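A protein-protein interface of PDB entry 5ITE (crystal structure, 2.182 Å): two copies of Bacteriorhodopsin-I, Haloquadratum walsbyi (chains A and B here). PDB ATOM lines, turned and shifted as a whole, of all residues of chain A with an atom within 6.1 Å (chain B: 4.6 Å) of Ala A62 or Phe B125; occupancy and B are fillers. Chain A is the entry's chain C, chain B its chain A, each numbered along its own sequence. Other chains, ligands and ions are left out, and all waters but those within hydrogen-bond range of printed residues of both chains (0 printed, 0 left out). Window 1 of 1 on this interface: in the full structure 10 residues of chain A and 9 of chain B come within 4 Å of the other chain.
Printed residues of chain B that touch a printed residue of chain A: Phe B125, Phe B145 and Ile B148. Hydrophobic or aromatic side chains of chain B that line the printed part of chain A: Phe B125, Phe B145 and Ile B148. Along chain B the printed residues that touch a printed residue of chain A span positions 125 to 148. Among the printed residues, 7 pairs touch across the chains.
Of the printed residues of chain B, Ala A58 touches Phe B125 (3.5 Å). Printed residues of chain B within 4 Å of Ile A59: Phe B125 (3.8 Å). Of chain B, only Phe B125 (3.8 Å) and Phe B145 (3.4 Å) come within 4 Å of Ala A62. Of the printed residues of chain B, Ser A66 touches Phe B145 (3.5 Å). Phe B125 touches three residues of chain A. Printed residues of chain A within 4 Å of Phe B145: Ala A62 (3.4 Å), Leu A65 (3.6 Å) and Ser A66 (3.5 Å). The nearest residue of chain B that does not touch Ala A62 is Thr B129 (4.03 Å). The nearest residue of chain A that does not touch Phe B125 is Leu A55 (4.6 Å).
The backbone carbonyl oxygen (O) of Ser A63 lies within hydrogen-bond range of the side-chain hydroxyl (OG) of Ser A66 (2.7 Å). The backbone NH of Leu A65 sits at hydrogen-bond distance from the side-chain hydroxyl of Thr A24 (3.4 Å). The backbone carbonyl oxygen of Phe B125 is in hydrogen-bond range of the side-chain hydroxyl of Thr B129. OG of Ser B152 lies within hydrogen-bond range of O of Ile B148 (3.5 Å).
Ala A58 touches Phe B125 (O to CE2, 3.5 Å). Ile A59 touches Phe B125 (CA to CE2, 3.8 Å). CZ of Phe B125 touches CB of Ala A62, 3.8 Å away. Phe B145 touches Ala A62 (CZ to O, 3.4 Å). Leu A65 touches Phe B145 (CD2 to CE1, 3.6 Å). Leu A65 touches Ile B148 (CD2 to CD1, 3.5 Å). Phe B145 touches Ser A66 (CZ to N, 3.5 Å).
No position is printed for both chains.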
ATOM      1  N   THR A  24      14.668  15.650 -33.441  1.00  0.00           N
ATOM      2  CA  THR A  24      15.502  14.563 -32.893  1.00  0.00           C
ATOM      3  C   THR A  24      16.991  14.771 -33.173  1.00  0.00           C
ATOM      4  O   THR A  24      17.821  14.752 -32.256  1.00  0.00           O
ATOM      5  CB  THR A  24      15.100  13.173 -33.431  1.00  0.00           C
ATOM      6  OG1 THR A  24      13.692  12.982 -33.266  1.00  0.00           O
ATOM      7  CG2 THR A  24      15.835  12.076 -32.645  1.00  0.00           C
ATOM      8  N   LEU A  55      21.907  16.419 -20.128  1.00  0.00           N
ATOM      9  CA  LEU A  55      20.688  15.649 -19.851  1.00  0.00           C
ATOM     10  C   LEU A  55      19.442  16.272 -20.490  1.00  0.00           C
ATOM     11  O   LEU A  55      18.555  15.557 -20.959  1.00  0.00           O
ATOM     12  CB  LEU A  55      20.472  15.486 -18.339  1.00  0.00           C
ATOM     13  CG  LEU A  55      19.290  14.603 -17.908  1.00  0.00           C
ATOM     14  CD1 LEU A  55      19.408  13.169 -18.434  1.00  0.00           C
ATOM     15  CD2 LEU A  55      19.136  14.591 -16.380  1.00  0.00           C
ATOM     16  N   PRO A  57      18.986  18.043 -23.563  1.00  0.00           N
ATOM     17  CA  PRO A  57      18.705  17.573 -24.924  1.00  0.00           C
ATOM     18  C   PRO A  57      18.732  16.062 -25.088  1.00  0.00           C
ATOM     19  O   PRO A  57      18.142  15.612 -26.042  1.00  0.00           O
ATOM     20  CB  PRO A  57      19.831  18.189 -25.763  1.00  0.00           C
ATOM     21  CG  PRO A  57      20.909  18.490 -24.799  1.00  0.00           C
ATOM     22  CD  PRO A  57      20.294  18.710 -23.469  1.00  0.00           C
ATOM     23  N   ALA A  58      19.416  15.298 -24.247  1.00  0.00           N
ATOM     24  CA  ALA A  58      19.159  13.856 -24.225  1.00  0.00           C
ATOM     25  C   ALA A  58      17.659  13.515 -24.090  1.00  0.00           C
ATOM     26  O   ALA A  58      17.101  12.752 -24.890  1.00  0.00           O
ATOM     27  CB  ALA A  58      19.938  13.210 -23.105  1.00  0.00           C
ATOM     28  N   ILE A  59      17.020  14.097 -23.078  1.00  0.00           N
ATOM     29  CA  ILE A  59      15.609  13.851 -22.789  1.00  0.00           C
ATOM     30  C   ILE A  59      14.765  14.338 -23.967  1.00  0.00           C
ATOM     31  O   ILE A  59      13.891  13.621 -24.477  1.00  0.00           O
ATOM     32  CB  ILE A  59      15.147  14.559 -21.494  1.00  0.00           C
ATOM     33  CG1 ILE A  59      15.756  13.895 -20.259  1.00  0.00           C
ATOM     34  CG2 ILE A  59      13.620  14.624 -21.428  1.00  0.00           C
ATOM     35  CD1 ILE A  59      15.873  14.814 -19.072  1.00  0.00           C
ATOM     36  N   ALA A  60      15.079  15.536 -24.458  1.00  0.00           N
ATOM     37  CA  ALA A  60      14.274  16.084 -25.545  1.00  0.00           C
ATOM     38  C   ALA A  60      14.436  15.251 -26.836  1.00  0.00           C
ATOM     39  O   ALA A  60      13.464  15.012 -27.557  1.00  0.00           O
ATOM     40  CB  ALA A  60      14.646  17.526 -25.795  1.00  0.00           C
ATOM     41  N   ALA A  61      15.647  14.778 -27.099  1.00  0.00           N
ATOM     42  CA  ALA A  61      15.905  13.911 -28.240  1.00  0.00           C
ATOM     43  C   ALA A  61      15.118  12.603 -28.130  1.00  0.00           C
ATOM     44  O   ALA A  61      14.545  12.139 -29.115  1.00  0.00           O
ATOM     45  CB  ALA A  61      17.405  13.626 -28.364  1.00  0.00           C
ATOM     46  N   ALA A  62      15.117  11.991 -26.946  1.00  0.00           N
ATOM     47  CA  ALA A  62      14.380  10.738 -26.785  1.00  0.00           C
ATOM     48  C   ALA A  62      12.871  10.974 -26.993  1.00  0.00           C
ATOM     49  O   ALA A  62      12.175  10.145 -27.597  1.00  0.00           O
ATOM     50  CB  ALA A  62      14.650  10.107 -25.401  1.00  0.00           C
ATOM     51  N   SER A  63      12.387  12.111 -26.490  1.00  0.00           N
ATOM     52  CA  SER A  63      10.990  12.531 -26.657  1.00  0.00           C
ATOM     53  C   SER A  63      10.582  12.706 -28.127  1.00  0.00           C
ATOM     54  O   SER A  63       9.593  12.124 -28.599  1.00  0.00           O
ATOM     55  CB  SER A  63      10.745  13.832 -25.888  1.00  0.00           C
ATOM     56  OG  SER A  63       9.401  14.259 -26.051  1.00  0.00           O
ATOM     57  N   TYR A  64      11.354  13.516 -28.838  1.00  0.00           N
ATOM     58  CA  TYR A  64      11.204  13.667 -30.280  1.00  0.00           C
ATOM     59  C   TYR A  64      11.226  12.344 -30.999  1.00  0.00           C
ATOM     60  O   TYR A  64      10.417  12.121 -31.891  1.00  0.00           O
ATOM     61  CB  TYR A  64      12.236  14.653 -30.842  1.00  0.00           C
ATOM     62  CG  TYR A  64      11.697  16.057 -30.769  1.00  0.00           C
ATOM     63  CD1 TYR A  64      11.711  16.785 -29.583  1.00  0.00           C
ATOM     64  CD2 TYR A  64      11.146  16.656 -31.904  1.00  0.00           C
ATOM     65  CE1 TYR A  64      11.183  18.074 -29.529  1.00  0.00           C
ATOM     66  CE2 TYR A  64      10.629  17.935 -31.861  1.00  0.00           C
ATOM     67  CZ  TYR A  64      10.649  18.641 -30.669  1.00  0.00           C
ATOM     68  OH  TYR A  64      10.131  19.916 -30.624  1.00  0.00           O
ATOM     69  N   LEU A  65      12.179  11.491 -30.672  1.00  0.00           N
ATOM     70  CA  LEU A  65      12.216  10.196 -31.330  1.00  0.00           C
ATOM     71  C   LEU A  65      10.935   9.398 -31.050  1.00  0.00           C
ATOM     72  O   LEU A  65      10.389   8.762 -31.958  1.00  0.00           O
ATOM     73  CB  LEU A  65      13.433   9.402 -30.875  1.00  0.00           C
ATOM     74  CG  LEU A  65      13.570   8.069 -31.597  1.00  0.00           C
ATOM     75  CD1 LEU A  65      13.873   8.352 -33.068  1.00  0.00           C
ATOM     76  CD2 LEU A  65      14.653   7.260 -30.966  1.00  0.00           C
ATOM     77  N   SER A  66      10.445   9.443 -29.810  1.00  0.00           N
ATOM     78  CA  SER A  66       9.224   8.711 -29.462  1.00  0.00           C
ATOM     79  C   SER A  66       8.044   9.236 -30.291  1.00  0.00           C
ATOM     80  O   SER A  66       7.227   8.450 -30.794  1.00  0.00           O
ATOM     81  CB  SER A  66       8.912   8.790 -27.957  1.00  0.00           C
ATOM     82  OG  SER A  66       8.279  10.011 -27.601  1.00  0.00           O
ATOM     83  N   MET A  67       7.951  10.558 -30.425  1.00  0.00           N
ATOM     84  CA  MET A  67       6.888  11.148 -31.230  1.00  0.00           C
ATOM     85  C   MET A  67       7.025  10.799 -32.721  1.00  0.00           C
ATOM     86  O   MET A  67       6.019  10.545 -33.398  1.00  0.00           O
ATOM     87  CB  MET A  67       6.855  12.663 -31.043  1.00  0.00           C
ATOM     88  CG  MET A  67       6.559  13.075 -29.611  1.00  0.00           C
ATOM     89  SD  MET A  67       6.414  14.853 -29.372  1.00  0.00           S
ATOM     90  CE  MET A  67       8.121  15.310 -29.092  1.00  0.00           C
ATOM     91  N   GLY B 121      19.559  10.973 -12.418  1.00  0.00           N
ATOM     92  CA  GLY B 121      19.097  11.495 -13.694  1.00  0.00           C
ATOM     93  C   GLY B 121      19.290  10.500 -14.821  1.00  0.00           C
ATOM     94  O   GLY B 121      18.371  10.237 -15.635  1.00  0.00           O
ATOM     95  N   ILE B 122      20.482   9.906 -14.843  1.00  0.00           N
ATOM     96  CA  ILE B 122      20.783   8.930 -15.885  1.00  0.00           C
ATOM     97  C   ILE B 122      19.922   7.670 -15.748  1.00  0.00           C
ATOM     98  O   ILE B 122      19.448   7.137 -16.729  1.00  0.00           O
ATOM     99  CB  ILE B 122      22.266   8.532 -15.852  1.00  0.00           C
ATOM    100  CG1 ILE B 122      23.145   9.757 -16.124  1.00  0.00           C
ATOM    101  CG2 ILE B 122      22.550   7.420 -16.870  1.00  0.00           C
ATOM    102  CD1 ILE B 122      24.629   9.479 -15.997  1.00  0.00           C
ATOM    103  N   ASP B 123      19.723   7.224 -14.514  1.00  0.00           N
ATOM    104  CA  ASP B 123      18.898   6.083 -14.158  1.00  0.00           C
ATOM    105  C   ASP B 123      17.463   6.266 -14.586  1.00  0.00           C
ATOM    106  O   ASP B 123      16.881   5.382 -15.218  1.00  0.00           O
ATOM    107  CB  ASP B 123      18.960   5.842 -12.655  1.00  0.00           C
ATOM    108  CG  ASP B 123      18.145   4.636 -12.223  1.00  0.00           C
ATOM    109  OD1 ASP B 123      18.711   3.522 -12.218  1.00  0.00           O
ATOM    110  OD2 ASP B 123      16.952   4.813 -11.865  1.00  0.00           O
ATOM    111  N   ALA B 124      16.886   7.396 -14.183  1.00  0.00           N
ATOM    112  CA  ALA B 124      15.547   7.787 -14.616  1.00  0.00           C
ATOM    113  C   ALA B 124      15.419   7.750 -16.135  1.00  0.00           C
ATOM    114  O   ALA B 124      14.460   7.160 -16.658  1.00  0.00           O
ATOM    115  CB  ALA B 124      15.212   9.186 -14.096  1.00  0.00           C
ATOM    116  N   PHE B 125      16.379   8.368 -16.837  1.00  0.00           N
ATOM    117  CA  PHE B 125      16.390   8.299 -18.307  1.00  0.00           C
ATOM    118  C   PHE B 125      16.352   6.840 -18.787  1.00  0.00           C
ATOM    119  O   PHE B 125      15.544   6.458 -19.679  1.00  0.00           O
ATOM    120  CB  PHE B 125      17.622   9.002 -18.879  1.00  0.00           C
ATOM    121  CG  PHE B 125      17.616   9.118 -20.380  1.00  0.00           C
ATOM    122  CD1 PHE B 125      18.248   8.172 -21.167  1.00  0.00           C
ATOM    123  CD2 PHE B 125      16.980  10.175 -21.002  1.00  0.00           C
ATOM    124  CE1 PHE B 125      18.246   8.279 -22.563  1.00  0.00           C
ATOM    125  CE2 PHE B 125      16.971  10.293 -22.396  1.00  0.00           C
ATOM    126  CZ  PHE B 125      17.604   9.352 -23.171  1.00  0.00           C
ATOM    127  N   MET B 126      17.210   6.018 -18.177  1.00  0.00           N
ATOM    128  CA  MET B 126      17.260   4.592 -18.491  1.00  0.00           C
ATOM    129  C   MET B 126      15.907   3.855 -18.326  1.00  0.00           C
ATOM    130  O   MET B 126      15.444   3.187 -19.265  1.00  0.00           O
ATOM    131  CB  MET B 126      18.337   3.914 -17.635  1.00  0.00           C
ATOM    132  CG  MET B 126      18.437   2.403 -17.845  1.00  0.00           C
ATOM    133  SD  MET B 126      19.528   1.505 -16.699  1.00  0.00           S
ATOM    134  CE  MET B 126      18.571   1.587 -15.163  1.00  0.00           C
ATOM    135  N   ILE B 127      15.241   4.044 -17.181  1.00  0.00           N
ATOM    136  CA  ILE B 127      13.945   3.402 -16.923  1.00  0.00           C
ATOM    137  C   ILE B 127      12.832   3.920 -17.830  1.00  0.00           C
ATOM    138  O   ILE B 127      12.089   3.136 -18.402  1.00  0.00           O
ATOM    139  CB  ILE B 127      13.473   3.600 -15.441  1.00  0.00           C
ATOM    140  CG1 ILE B 127      14.468   2.990 -14.451  1.00  0.00           C
ATOM    141  CG2 ILE B 127      12.081   3.014 -15.220  1.00  0.00           C
ATOM    142  CD1 ILE B 127      14.798   1.526 -14.731  1.00  0.00           C
ATOM    143  N   VAL B 128      12.732   5.231 -18.007  1.00  0.00           N
ATOM    144  CA  VAL B 128      11.694   5.741 -18.897  1.00  0.00           C
ATOM    145  C   VAL B 128      11.867   5.316 -20.376  1.00  0.00           C
ATOM    146  O   VAL B 128      10.878   4.918 -21.030  1.00  0.00           O
ATOM    147  CB  VAL B 128      11.624   7.272 -18.773  1.00  0.00           C
ATOM    148  CG1 VAL B 128      10.506   7.857 -19.639  1.00  0.00           C
ATOM    149  CG2 VAL B 128      11.424   7.637 -17.319  1.00  0.00           C
ATOM    150  N   THR B 129      13.096   5.364 -20.903  1.00  0.00           N
ATOM    151  CA  THR B 129      13.305   4.941 -22.293  1.00  0.00           C
ATOM    152  C   THR B 129      13.110   3.434 -22.433  1.00  0.00           C
ATOM    153  O   THR B 129      12.632   2.949 -23.472  1.00  0.00           O
ATOM    154  CB  THR B 129      14.705   5.317 -22.833  1.00  0.00           C
ATOM    155  OG1 THR B 129      15.720   4.853 -21.936  1.00  0.00           O
ATOM    156  CG2 THR B 129      14.822   6.844 -23.040  1.00  0.00           C
ATOM    157  N   PHE B 145      14.779   2.043 -28.813  1.00  0.00           N
ATOM    158  CA  PHE B 145      14.679   2.487 -27.425  1.00  0.00           C
ATOM    159  C   PHE B 145      15.325   1.499 -26.469  1.00  0.00           C
ATOM    160  O   PHE B 145      15.825   1.900 -25.417  1.00  0.00           O
ATOM    161  CB  PHE B 145      13.242   2.804 -27.056  1.00  0.00           C
ATOM    162  CG  PHE B 145      12.849   4.183 -27.459  1.00  0.00           C
ATOM    163  CD1 PHE B 145      12.323   4.420 -28.719  1.00  0.00           C
ATOM    164  CD2 PHE B 145      13.072   5.255 -26.619  1.00  0.00           C
ATOM    165  CE1 PHE B 145      11.981   5.700 -29.121  1.00  0.00           C
ATOM    166  CE2 PHE B 145      12.738   6.551 -27.016  1.00  0.00           C
ATOM    167  CZ  PHE B 145      12.184   6.766 -28.276  1.00  0.00           C
ATOM    168  N   ILE B 148      18.909   2.694 -26.862  1.00  0.00           N
ATOM    169  CA  ILE B 148      19.078   3.939 -26.098  1.00  0.00           C
ATOM    170  C   ILE B 148      19.174   3.665 -24.590  1.00  0.00           C
ATOM    171  O   ILE B 148      20.081   4.162 -23.875  1.00  0.00           O
ATOM    172  CB  ILE B 148      17.905   4.924 -26.371  1.00  0.00           C
ATOM    173  CG1 ILE B 148      18.011   5.507 -27.785  1.00  0.00           C
ATOM    174  CG2 ILE B 148      17.876   6.067 -25.353  1.00  0.00           C
ATOM    175  CD1 ILE B 148      16.671   5.958 -28.366  1.00  0.00           C
ATOM    176  N   SER B 152      22.459   4.101 -22.068  1.00  0.00           N
ATOM    177  CA  SER B 152      22.374   4.877 -20.838  1.00  0.00           C
ATOM    178  C   SER B 152      22.772   4.005 -19.647  1.00  0.00           C
ATOM    179  O   SER B 152      23.468   4.469 -18.766  1.00  0.00           O
ATOM    180  CB  SER B 152      20.974   5.476 -20.642  1.00  0.00           C
ATOM    181  OG  SER B 152      19.997   4.476 -20.435  1.00  0.00           O
